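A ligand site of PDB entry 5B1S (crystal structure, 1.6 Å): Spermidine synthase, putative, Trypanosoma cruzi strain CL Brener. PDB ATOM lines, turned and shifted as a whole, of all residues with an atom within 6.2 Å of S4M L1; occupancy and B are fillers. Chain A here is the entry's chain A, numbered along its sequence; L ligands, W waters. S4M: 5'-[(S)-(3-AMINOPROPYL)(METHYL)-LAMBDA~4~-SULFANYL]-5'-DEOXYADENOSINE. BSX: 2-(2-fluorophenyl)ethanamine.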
ATOM      1  N   GLN A  48     -28.640  30.086  -5.798  1.00  0.00           N
ATOM      2  CA  GLN A  48     -27.346  30.665  -6.255  1.00  0.00           C
ATOM      3  C   GLN A  48     -27.602  31.813  -7.186  1.00  0.00           C
ATOM      4  O   GLN A  48     -28.646  31.869  -7.830  1.00  0.00           O
ATOM      5  CB  GLN A  48     -26.561  29.552  -7.027  1.00  0.00           C
ATOM      6  CG  GLN A  48     -26.138  28.407  -6.100  1.00  0.00           C
ATOM      7  CD  GLN A  48     -25.632  27.212  -6.854  1.00  0.00           C
ATOM      8  OE1 GLN A  48     -24.443  26.814  -6.667  1.00  0.00           O
ATOM      9  NE2 GLN A  48     -26.483  26.588  -7.705  1.00  0.00           N
ATOM     10  N   MET A  65     -20.908  30.416 -18.259  1.00  0.00           N
ATOM     11  CA  MET A  65     -21.788  30.371 -17.129  1.00  0.00           C
ATOM     12  C   MET A  65     -21.066  30.594 -15.846  1.00  0.00           C
ATOM     13  O   MET A  65     -20.005  29.941 -15.611  1.00  0.00           O
ATOM     14  CB  MET A  65     -22.540  29.012 -17.100  1.00  0.00           C
ATOM     15  CG  MET A  65     -23.559  29.005 -15.974  1.00  0.00           C
ATOM     16  SD  MET A  65     -24.846  27.782 -16.299  1.00  0.00           S
ATOM     17  CE  MET A  65     -23.815  26.922 -15.282  1.00  0.00           C
ATOM     18  N   LEU A  67     -21.763  30.713 -11.330  1.00  0.00           N
ATOM     19  CA  LEU A  67     -22.638  30.521 -10.175  1.00  0.00           C
ATOM     20  C   LEU A  67     -21.987  31.230  -9.027  1.00  0.00           C
ATOM     21  O   LEU A  67     -20.890  30.954  -8.629  1.00  0.00           O
ATOM     22  CB  LEU A  67     -22.888  29.039  -9.843  1.00  0.00           C
ATOM     23  CG  LEU A  67     -23.791  28.338 -10.829  1.00  0.00           C
ATOM     24  CD1 LEU A  67     -23.753  26.795 -10.589  1.00  0.00           C
ATOM     25  CD2 LEU A  67     -25.201  28.768 -10.572  1.00  0.00           C
ATOM     26  N   GLN A  72     -18.201  28.520 -14.257  1.00  0.00           N
ATOM     27  CA  GLN A  72     -18.506  27.057 -14.226  1.00  0.00           C
ATOM     28  C   GLN A  72     -18.116  26.341 -15.499  1.00  0.00           C
ATOM     29  O   GLN A  72     -17.611  25.200 -15.460  1.00  0.00           O
ATOM     30  CB  GLN A  72     -20.013  26.790 -13.936  1.00  0.00           C
ATOM     31  CG  GLN A  72     -20.421  27.426 -12.627  1.00  0.00           C
ATOM     32  CD  GLN A  72     -19.883  26.724 -11.421  1.00  0.00           C
ATOM     33  OE1 GLN A  72     -20.156  25.553 -11.230  1.00  0.00           O
ATOM     34  NE2 GLN A  72     -19.187  27.432 -10.563  1.00  0.00           N
ATOM     35  N   VAL A  73     -18.497  26.882 -16.645  1.00  0.00           N
ATOM     36  CA  VAL A  73     -18.270  26.344 -17.937  1.00  0.00           C
ATOM     37  C   VAL A  73     -18.077  27.454 -18.954  1.00  0.00           C
ATOM     38  O   VAL A  73     -18.657  28.512 -18.808  1.00  0.00           O
ATOM     39  CB  VAL A  73     -19.414  25.447 -18.466  1.00  0.00           C
ATOM     40  CG1 VAL A  73     -19.585  24.137 -17.646  1.00  0.00           C
ATOM     41  CG2 VAL A  73     -20.728  26.169 -18.517  1.00  0.00           C
ATOM     42  N   TYR A  81     -12.690  19.199 -18.299  1.00  0.00           N
ATOM     43  CA  TYR A  81     -13.138  18.662 -17.041  1.00  0.00           C
ATOM     44  C   TYR A  81     -14.207  17.613 -17.173  1.00  0.00           C
ATOM     45  O   TYR A  81     -14.203  16.586 -16.477  1.00  0.00           O
ATOM     46  CB  TYR A  81     -13.664  19.851 -16.258  1.00  0.00           C
ATOM     47  CG  TYR A  81     -14.352  19.581 -14.929  1.00  0.00           C
ATOM     48  CD1 TYR A  81     -13.598  19.468 -13.746  1.00  0.00           C
ATOM     49  CD2 TYR A  81     -15.776  19.535 -14.829  1.00  0.00           C
ATOM     50  CE1 TYR A  81     -14.216  19.267 -12.582  1.00  0.00           C
ATOM     51  CE2 TYR A  81     -16.426  19.259 -13.589  1.00  0.00           C
ATOM     52  CZ  TYR A  81     -15.644  19.136 -12.475  1.00  0.00           C
ATOM     53  OH  TYR A  81     -16.283  18.990 -11.260  1.00  0.00           O
ATOM     54  N   HIS A  82     -15.088  17.794 -18.158  1.00  0.00           N
ATOM     55  CA  HIS A  82     -16.085  16.759 -18.357  1.00  0.00           C
ATOM     56  C   HIS A  82     -15.550  15.397 -18.775  1.00  0.00           C
ATOM     57  O   HIS A  82     -15.951  14.344 -18.234  1.00  0.00           O
ATOM     58  CB  HIS A  82     -17.124  17.352 -19.343  1.00  0.00           C
ATOM     59  CG  HIS A  82     -17.881  18.436 -18.742  1.00  0.00           C
ATOM     60  ND1 HIS A  82     -18.316  19.499 -19.501  1.00  0.00           N
ATOM     61  CD2 HIS A  82     -18.263  18.680 -17.455  1.00  0.00           C
ATOM     62  CE1 HIS A  82     -18.935  20.361 -18.702  1.00  0.00           C
ATOM     63  NE2 HIS A  82     -18.926  19.882 -17.467  1.00  0.00           N
ATOM     64  N   ILE A 102     -23.483  13.689  -8.531  1.00  0.00           N
ATOM     65  CA  ILE A 102     -24.032  14.709  -7.624  1.00  0.00           C
ATOM     66  C   ILE A 102     -23.548  16.053  -8.152  1.00  0.00           C
ATOM     67  O   ILE A 102     -22.369  16.264  -8.476  1.00  0.00           O
ATOM     68  CB  ILE A 102     -23.437  14.507  -6.229  1.00  0.00           C
ATOM     69  CG1 ILE A 102     -23.895  13.107  -5.641  1.00  0.00           C
ATOM     70  CG2 ILE A 102     -23.896  15.705  -5.363  1.00  0.00           C
ATOM     71  CD1 ILE A 102     -22.908  12.456  -4.698  1.00  0.00           C
ATOM     72  N   GLY A 103     -24.483  17.009  -8.272  1.00  0.00           N
ATOM     73  CA  GLY A 103     -24.183  18.264  -8.990  1.00  0.00           C
ATOM     74  C   GLY A 103     -24.322  17.998 -10.486  1.00  0.00           C
ATOM     75  O   GLY A 103     -25.231  17.304 -10.920  1.00  0.00           O
ATOM     76  N   GLY A 104     -23.457  18.641 -11.245  1.00  0.00           N
ATOM     77  CA  GLY A 104     -23.345  18.342 -12.693  1.00  0.00           C
ATOM     78  C   GLY A 104     -24.615  18.716 -13.485  1.00  0.00           C
ATOM     79  O   GLY A 104     -24.909  18.125 -14.526  1.00  0.00           O
ATOM     80  N   GLY A 105     -25.366  19.667 -12.967  1.00  0.00           N
ATOM     81  CA  GLY A 105     -26.618  20.034 -13.638  1.00  0.00           C
ATOM     82  C   GLY A 105     -26.511  20.596 -15.017  1.00  0.00           C
ATOM     83  O   GLY A 105     -27.528  20.642 -15.731  1.00  0.00           O
ATOM     84  N   ASP A 106     -25.319  21.004 -15.454  1.00  0.00           N
ATOM     85  CA  ASP A 106     -25.125  21.311 -16.868  1.00  0.00           C
ATOM     86  C   ASP A 106     -25.182  20.154 -17.820  1.00  0.00           C
ATOM     87  O   ASP A 106     -25.419  20.334 -19.054  1.00  0.00           O
ATOM     88  CB  ASP A 106     -23.818  22.068 -17.038  1.00  0.00           C
ATOM     89  CG  ASP A 106     -22.699  21.308 -16.375  1.00  0.00           C
ATOM     90  OD1 ASP A 106     -22.242  20.355 -16.903  1.00  0.00           O
ATOM     91  OD2 ASP A 106     -22.329  21.691 -15.249  1.00  0.00           O
ATOM     92  N   GLY A 107     -24.957  18.930 -17.283  1.00  0.00           N
ATOM     93  CA  GLY A 107     -25.019  17.692 -18.008  1.00  0.00           C
ATOM     94  C   GLY A 107     -23.740  17.238 -18.681  1.00  0.00           C
ATOM     95  O   GLY A 107     -23.701  16.189 -19.296  1.00  0.00           O
ATOM     96  N   GLY A 108     -22.653  18.009 -18.538  1.00  0.00           N
ATOM     97  CA  GLY A 108     -21.386  17.657 -19.248  1.00  0.00           C
ATOM     98  C   GLY A 108     -20.783  16.330 -18.841  1.00  0.00           C
ATOM     99  O   GLY A 108     -20.342  15.526 -19.645  1.00  0.00           O
ATOM    100  N   VAL A 109     -20.674  16.136 -17.493  1.00  0.00           N
ATOM    101  CA  VAL A 109     -20.135  14.778 -17.080  1.00  0.00           C
ATOM    102  C   VAL A 109     -21.082  13.692 -17.549  1.00  0.00           C
ATOM    103  O   VAL A 109     -20.603  12.659 -17.978  1.00  0.00           O
ATOM    104  CB  VAL A 109     -19.922  14.751 -15.532  1.00  0.00           C
ATOM    105  CG1 VAL A 109     -19.565  13.318 -14.978  1.00  0.00           C
ATOM    106  CG2 VAL A 109     -18.837  15.779 -15.130  1.00  0.00           C
ATOM    107  N   VAL A 125     -28.217  14.294  -9.532  1.00  0.00           N
ATOM    108  CA  VAL A 125     -29.000  15.053  -8.522  1.00  0.00           C
ATOM    109  C   VAL A 125     -28.270  16.346  -8.293  1.00  0.00           C
ATOM    110  O   VAL A 125     -27.130  16.367  -7.773  1.00  0.00           O
ATOM    111  CB  VAL A 125     -29.087  14.246  -7.200  1.00  0.00           C
ATOM    112  CG1 VAL A 125     -29.934  15.037  -6.191  1.00  0.00           C
ATOM    113  CG2 VAL A 125     -29.767  12.876  -7.500  1.00  0.00           C
ATOM    114  N   ASP A 126     -28.921  17.466  -8.668  1.00  0.00           N
ATOM    115  CA  ASP A 126     -28.360  18.843  -8.572  1.00  0.00           C
ATOM    116  C   ASP A 126     -29.378  19.646  -7.838  1.00  0.00           C
ATOM    117  O   ASP A 126     -30.551  19.460  -8.065  1.00  0.00           O
ATOM    118  CB  ASP A 126     -28.085  19.408  -9.955  1.00  0.00           C
ATOM    119  CG  ASP A 126     -27.251  20.667  -9.914  1.00  0.00           C
ATOM    120  OD1 ASP A 126     -27.648  21.604  -9.185  1.00  0.00           O
ATOM    121  OD2 ASP A 126     -26.170  20.735 -10.506  1.00  0.00           O
ATOM    122  N   ILE A 127     -28.900  20.428  -6.905  1.00  0.00           N
ATOM    123  CA  ILE A 127     -29.780  21.212  -6.047  1.00  0.00           C
ATOM    124  C   ILE A 127     -30.527  22.317  -6.756  1.00  0.00           C
ATOM    125  O   ILE A 127     -31.616  22.734  -6.258  1.00  0.00           O
ATOM    126  CB  ILE A 127     -29.018  21.734  -4.812  1.00  0.00           C
ATOM    127  CG1 ILE A 127     -29.974  22.043  -3.673  1.00  0.00           C
ATOM    128  CG2 ILE A 127     -28.093  22.924  -5.101  1.00  0.00           C
ATOM    129  CD1 ILE A 127     -29.176  22.524  -2.468  1.00  0.00           C
ATOM    130  N   ASP A 128     -30.082  22.725  -7.938  1.00  0.00           N
ATOM    131  CA  ASP A 128     -30.581  23.964  -8.574  1.00  0.00           C
ATOM    132  C   ASP A 128     -31.175  23.681  -9.935  1.00  0.00           C
ATOM    133  O   ASP A 128     -30.494  23.520 -10.969  1.00  0.00           O
ATOM    134  CB  ASP A 128     -29.427  24.973  -8.631  1.00  0.00           C
ATOM    135  CG  ASP A 128     -29.910  26.368  -8.921  1.00  0.00           C
ATOM    136  OD1 ASP A 128     -30.969  26.504  -9.593  1.00  0.00           O
ATOM    137  OD2 ASP A 128     -29.168  27.281  -8.494  1.00  0.00           O
ATOM    138  N   VAL A 131     -30.222  25.651 -13.080  1.00  0.00           N
ATOM    139  CA  VAL A 131     -29.037  25.337 -13.861  1.00  0.00           C
ATOM    140  C   VAL A 131     -29.299  24.379 -15.024  1.00  0.00           C
ATOM    141  O   VAL A 131     -28.815  24.534 -16.134  1.00  0.00           O
ATOM    142  CB  VAL A 131     -27.912  24.742 -12.922  1.00  0.00           C
ATOM    143  CG1 VAL A 131     -26.671  24.257 -13.697  1.00  0.00           C
ATOM    144  CG2 VAL A 131     -27.501  25.741 -11.853  1.00  0.00           C
ATOM    145  N   MET A 132     -30.095  23.317 -14.797  1.00  0.00           N
ATOM    146  CA  MET A 132     -30.471  22.404 -15.871  1.00  0.00           C
ATOM    147  C   MET A 132     -31.267  23.132 -16.905  1.00  0.00           C
ATOM    148  O   MET A 132     -30.985  22.915 -18.064  1.00  0.00           O
ATOM    149  CB  MET A 132     -31.239  21.137 -15.460  1.00  0.00           C
ATOM    150  CG  MET A 132     -30.413  20.129 -14.635  1.00  0.00           C
ATOM    151  SD  MET A 132     -30.075  20.593 -12.936  1.00  0.00           S
ATOM    152  CE  MET A 132     -31.120  19.567 -11.885  1.00  0.00           C
ATOM    153  N   GLY A 156     -32.459  18.242  -6.118  1.00  0.00           N
ATOM    154  CA  GLY A 156     -32.385  18.107  -4.669  1.00  0.00           C
ATOM    155  C   GLY A 156     -30.953  18.205  -4.166  1.00  0.00           C
ATOM    156  O   GLY A 156     -30.024  18.217  -4.975  1.00  0.00           O
ATOM    157  N   ASP A 157     -30.786  18.284  -2.847  1.00  0.00           N
ATOM    158  CA  ASP A 157     -29.484  18.378  -2.238  1.00  0.00           C
ATOM    159  C   ASP A 157     -28.885  16.997  -2.285  1.00  0.00           C
ATOM    160  O   ASP A 157     -29.496  15.982  -1.839  1.00  0.00           O
ATOM    161  CB  ASP A 157     -29.690  18.868  -0.817  1.00  0.00           C
ATOM    162  CG  ASP A 157     -28.408  19.131  -0.084  1.00  0.00           C
ATOM    163  OD1 ASP A 157     -27.327  18.795  -0.519  1.00  0.00           O
ATOM    164  OD2 ASP A 157     -28.493  19.679   1.043  1.00  0.00           O
ATOM    165  N   GLY A 158     -27.669  16.941  -2.866  1.00  0.00           N
ATOM    166  CA  GLY A 158     -26.934  15.690  -2.914  1.00  0.00           C
ATOM    167  C   GLY A 158     -26.627  15.088  -1.552  1.00  0.00           C
ATOM    168  O   GLY A 158     -26.489  13.866  -1.438  1.00  0.00           O
ATOM    169  N   LEU A 159     -26.463  15.909  -0.497  1.00  0.00           N
ATOM    170  CA  LEU A 159     -26.232  15.387   0.814  1.00  0.00           C
ATOM    171  C   LEU A 159     -27.379  14.456   1.314  1.00  0.00           C
ATOM    172  O   LEU A 159     -27.103  13.417   1.909  1.00  0.00           O
ATOM    173  CB  LEU A 159     -26.125  16.551   1.788  1.00  0.00           C
ATOM    174  CG  LEU A 159     -25.517  16.217   3.159  1.00  0.00           C
ATOM    175  CD1 LEU A 159     -23.994  16.019   3.124  1.00  0.00           C
ATOM    176  CD2 LEU A 159     -25.869  17.332   4.136  1.00  0.00           C
ATOM    177  N   ASP A 176     -19.662  16.460  -8.908  1.00  0.00           N
ATOM    178  CA  ASP A 176     -19.340  17.630  -9.708  1.00  0.00           C
ATOM    179  C   ASP A 176     -19.975  18.828  -9.149  1.00  0.00           C
ATOM    180  O   ASP A 176     -21.067  19.191  -9.604  1.00  0.00           O
ATOM    181  CB  ASP A 176     -19.771  17.381 -11.173  1.00  0.00           C
ATOM    182  CG  ASP A 176     -19.575  18.627 -12.065  1.00  0.00           C
ATOM    183  OD1 ASP A 176     -18.883  19.534 -11.650  1.00  0.00           O
ATOM    184  OD2 ASP A 176     -20.142  18.642 -13.185  1.00  0.00           O
ATOM    185  N   THR A 177     -19.326  19.433  -8.115  1.00  0.00           N
ATOM    186  CA  THR A 177     -19.937  20.530  -7.358  1.00  0.00           C
ATOM    187  C   THR A 177     -19.257  21.880  -7.589  1.00  0.00           C
ATOM    188  O   THR A 177     -18.091  22.015  -7.996  1.00  0.00           O
ATOM    189  CB  THR A 177     -19.786  20.314  -5.818  1.00  0.00           C
ATOM    190  OG1 THR A 177     -18.389  20.414  -5.497  1.00  0.00           O
ATOM    191  CG2 THR A 177     -20.307  18.876  -5.414  1.00  0.00           C
ATOM    192  N   THR A 178     -20.012  22.896  -7.240  1.00  0.00           N
ATOM    193  CA  THR A 178     -19.375  24.190  -7.045  1.00  0.00           C
ATOM    194  C   THR A 178     -18.387  24.262  -5.867  1.00  0.00           C
ATOM    195  O   THR A 178     -18.127  23.288  -5.150  1.00  0.00           O
ATOM    196  CB  THR A 178     -20.545  25.197  -6.790  1.00  0.00           C
ATOM    197  OG1 THR A 178     -21.427  24.606  -5.799  1.00  0.00           O
ATOM    198  CG2 THR A 178     -21.341  25.444  -8.020  1.00  0.00           C
ATOM    199  N   GLY A 182     -21.198  28.232  -0.452  1.00  0.00           N
ATOM    200  CA  GLY A 182     -22.464  28.129  -1.099  1.00  0.00           C
ATOM    201  C   GLY A 182     -23.099  26.792  -0.776  1.00  0.00           C
ATOM    202  O   GLY A 182     -22.746  26.172   0.186  1.00  0.00           O
ATOM    203  N   PRO A 183     -24.016  26.369  -1.642  1.00  0.00           N
ATOM    204  CA  PRO A 183     -24.717  25.136  -1.327  1.00  0.00           C
ATOM    205  C   PRO A 183     -23.922  23.863  -1.363  1.00  0.00           C
ATOM    206  O   PRO A 183     -24.409  22.814  -0.845  1.00  0.00           O
ATOM    207  CB  PRO A 183     -25.856  25.148  -2.347  1.00  0.00           C
ATOM    208  CG  PRO A 183     -25.400  25.958  -3.465  1.00  0.00           C
ATOM    209  CD  PRO A 183     -24.577  27.040  -2.800  1.00  0.00           C
ATOM    210  N   ALA A 184     -22.692  23.948  -1.889  1.00  0.00           N
ATOM    211  CA  ALA A 184     -21.877  22.733  -1.873  1.00  0.00           C
ATOM    212  C   ALA A 184     -21.046  22.539  -0.630  1.00  0.00           C
ATOM    213  O   ALA A 184     -20.318  21.567  -0.488  1.00  0.00           O
ATOM    214  CB  ALA A 184     -20.969  22.768  -3.092  1.00  0.00           C
ATOM    215  N   SER A 185     -21.235  23.413   0.375  1.00  0.00           N
ATOM    216  CA  SER A 185     -20.337  23.414   1.496  1.00  0.00           C
ATOM    217  C   SER A 185     -20.174  22.071   2.177  1.00  0.00           C
ATOM    218  O   SER A 185     -19.043  21.590   2.400  1.00  0.00           O
ATOM    219  CB  SER A 185     -20.809  24.446   2.486  1.00  0.00           C
ATOM    220  OG  SER A 185     -19.962  24.376   3.634  1.00  0.00           O
ATOM    221  N   LEU A 187     -20.694  19.142   0.949  1.00  0.00           N
ATOM    222  CA  LEU A 187     -20.203  18.102   0.060  1.00  0.00           C
ATOM    223  C   LEU A 187     -18.666  18.058   0.000  1.00  0.00           C
ATOM    224  O   LEU A 187     -18.091  17.222  -0.729  1.00  0.00           O
ATOM    225  CB  LEU A 187     -20.705  18.346  -1.351  1.00  0.00           C
ATOM    226  CG  LEU A 187     -22.133  18.138  -1.596  1.00  0.00           C
ATOM    227  CD1 LEU A 187     -23.134  17.498  -0.641  1.00  0.00           C
ATOM    228  CD2 LEU A 187     -22.601  18.676  -2.906  1.00  0.00           C
ATOM    229  N   TYR A 245     -10.802  28.025 -15.133  1.00  0.00           N
ATOM    230  CA  TYR A 245     -10.901  27.875 -13.700  1.00  0.00           C
ATOM    231  C   TYR A 245      -9.711  28.584 -13.045  1.00  0.00           C
ATOM    232  O   TYR A 245      -8.742  28.808 -13.735  1.00  0.00           O
ATOM    233  CB  TYR A 245     -10.984  26.382 -13.243  1.00  0.00           C
ATOM    234  CG  TYR A 245     -12.203  25.669 -13.709  1.00  0.00           C
ATOM    235  CD1 TYR A 245     -13.461  26.334 -13.649  1.00  0.00           C
ATOM    236  CD2 TYR A 245     -12.148  24.378 -14.061  1.00  0.00           C
ATOM    237  CE1 TYR A 245     -14.660  25.648 -14.043  1.00  0.00           C
ATOM    238  CE2 TYR A 245     -13.296  23.698 -14.463  1.00  0.00           C
ATOM    239  CZ  TYR A 245     -14.535  24.337 -14.384  1.00  0.00           C
ATOM    240  OH  TYR A 245     -15.656  23.645 -14.826  1.00  0.00           O
HETATM  241  CA  S4M L   1     -18.844  21.995 -14.549  1.00  0.00           C
HETATM  242  N   S4M L   1     -19.766  20.851 -14.880  1.00  0.00           N
HETATM  243  CB  S4M L   1     -19.578  22.975 -13.680  1.00  0.00           C
HETATM  244  CG  S4M L   1     -19.993  22.446 -12.280  1.00  0.00           C
HETATM  245  SD  S4M L   1     -21.770  22.093 -12.143  1.00  0.00           S
HETATM  246  CE  S4M L   1     -22.465  23.737 -12.591  1.00  0.00           C
HETATM  247  C5' S4M L   1     -21.772  22.357 -10.312  1.00  0.00           C
HETATM  248  C4' S4M L   1     -23.156  22.186  -9.694  1.00  0.00           C
HETATM  249  O4' S4M L   1     -23.046  21.822  -8.281  1.00  0.00           O
HETATM  250  C1' S4M L   1     -24.400  22.025  -7.839  1.00  0.00           C
HETATM  251  C2' S4M L   1     -24.653  23.410  -8.462  1.00  0.00           C
HETATM  252  O2' S4M L   1     -26.080  23.659  -8.371  1.00  0.00           O
HETATM  253  C3' S4M L   1     -24.058  23.397  -9.853  1.00  0.00           C
HETATM  254  O3' S4M L   1     -25.103  23.175 -10.787  1.00  0.00           O
HETATM  255  N9  S4M L   1     -24.549  21.933  -6.416  1.00  0.00           N
HETATM  256  C8  S4M L   1     -24.076  22.754  -5.431  1.00  0.00           C
HETATM  257  N7  S4M L   1     -24.373  22.375  -4.242  1.00  0.00           N
HETATM  258  C5  S4M L   1     -25.111  21.194  -4.417  1.00  0.00           C
HETATM  259  C6  S4M L   1     -25.665  20.293  -3.506  1.00  0.00           C
HETATM  260  N6  S4M L   1     -25.683  20.445  -2.129  1.00  0.00           N
HETATM  261  C4  S4M L   1     -25.202  20.919  -5.751  1.00  0.00           C
HETATM  262  N3  S4M L   1     -25.790  19.839  -6.268  1.00  0.00           N
HETATM  263  C2  S4M L   1     -26.316  19.072  -5.321  1.00  0.00           C
HETATM  264  N1  S4M L   1     -26.317  19.210  -3.975  1.00  0.00           N
HETATM  265  C7  BSX L   2     -15.234  22.652 -11.721  1.00  0.00           C
HETATM  266  C9  BSX L   2     -16.603  22.572 -11.650  1.00  0.00           C
HETATM  267  C4  BSX L   2     -14.446  23.509 -10.965  1.00  0.00           C
HETATM  268  C6  BSX L   2     -17.212  23.456 -10.760  1.00  0.00           C
HETATM  269  C1  BSX L   2     -15.052  24.383 -10.055  1.00  0.00           C
HETATM  270  C3  BSX L   2     -16.424  24.314 -10.014  1.00  0.00           C
HETATM  271  C2  BSX L   2     -14.194  25.336  -9.212  1.00  0.00           C
HETATM  272  C5  BSX L   2     -14.205  26.697  -9.898  1.00  0.00           C
HETATM  273  N8  BSX L   2     -13.719  27.778  -8.994  1.00  0.00           N
HETATM  274  F10 BSX L   2     -17.096  25.167  -9.127  1.00  0.00           F
HETATM  275  O   HOH W   1     -21.389  18.173 -15.506  1.00  0.00           O
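The side-chain carboxylate (OD2) of Asp 128 lies within hydrogen-bond range of the side-chain amide nitrogen (NE2) of Gln 48, 2.9 Å away. The backbone NH (N) of Gly 156 is in hydrogen-bond range of the backbone carbonyl oxygen (O) of Asp 126. The backbone carbonyl oxygen of Gly 156 sits at hydrogen-bond distance from the backbone NH of Ile 127 (3.1 Å). The backbone carbonyl oxygen of Ile 102 sits at hydrogen-bond distance from the backbone NH of Asp 176. NE2 of His 82 sits at hydrogen-bond distance from OD1 of Asp 106, 3.4 Å away. OH of Tyr 81 is in hydrogen-bond range of OD1 of Asp 176. OD1 of Asp 106 sits at hydrogen-bond distance from N of Gly 108, 2.9 Å away. The backbone carbonyl oxygen (O) of Val 73 is in hydrogen-bond range of the backbone NH (N) of Met 65 (3.0 Å).
Water W1 lies within hydrogen-bond range of the side-chain carboxylate of Asp 176, the side-chain carboxylate of Asp 106, the backbone NH of Val 109, a nitrogen (N) of S4M L1 and the backbone NH of Gly 108.
Merely in contact with S4M L1: Leu 67 (3.5 Å), Gln 72 (3.2 Å), Val 73 (3.8 Å), Tyr 81 (3.8 Å), Gly 103 (3.5 Å), Gly 104 (3.9 Å), Val 125 (3.7 Å), Asp 128 (3.6 Å), Val 131 (3.5 Å), Gly 156 (3.8 Å), Thr 177 (3.5 Å), Leu 187 (3.5 Å) and Tyr 245 (3.6 Å). Hydrophobic or aromatic side chains within 4 Å of S4M L1: Leu 67, Val 73, Tyr 81, His 82, Ile 127, Val 131, Pro 183, Ala 184 and Leu 187. Within 4 Å of S4M L1: Gln 48, Leu 67, Gln 72, Val 73, Tyr 81, His 82, Gly 103, Gly 104, Asp 106, Val 125, Asp 126, Ile 127, Asp 128, Val 131, Gly 156, Asp 157, Gly 158, Asp 176, Thr 177, Thr 178, Pro 183, Ala 184, Leu 187 and Tyr 245. Along chain A the residues within 4 Å of S4M L1 span positions 48 to 245. The nearest printed residue that does not touch S4M L1 is Gly 105 (4.1 Å).
The backbone NH (N) of Thr 178 lies within hydrogen-bond range of an oxygen (O4') of S4M L1 (3.4 Å). O2' of S4M L1 sits at hydrogen-bond distance from NE2 of Gln 48, at 3.0 Å. A nitrogen (N6) of S4M L1 sits at hydrogen-bond distance from the side-chain carboxylate (OD1) of Asp 157 (2.8 Å). The side-chain carboxylate (OD2) of Asp 126 is in hydrogen-bond range of an oxygen (O3') of S4M L1, 2.7 Å away. N3 of S4M L1 is in hydrogen-bond range of N of Ile 127. N7 of S4M L1 sits at hydrogen-bond distance from N of Ala 184 (3.3 Å). A ring nitrogen (NE2) of His 82 sits at hydrogen-bond distance from a nitrogen (N) of S4M L1 (2.9 Å). The side-chain carboxylate (OD2) of Asp 106 lies within salt-bridge range of a nitrogen (N) of S4M L1. O of Pro 183 lies within hydrogen-bond range of N6 of S4M L1, at 3.0 Å. A nitrogen (N1) of S4M L1 is in hydrogen-bond range of the backbone NH of Gly 158 (2.9 Å). The side-chain carboxylate of Asp 176 lies within salt-bridge range of a nitrogen (N) of S4M L1 (2.8 Å).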
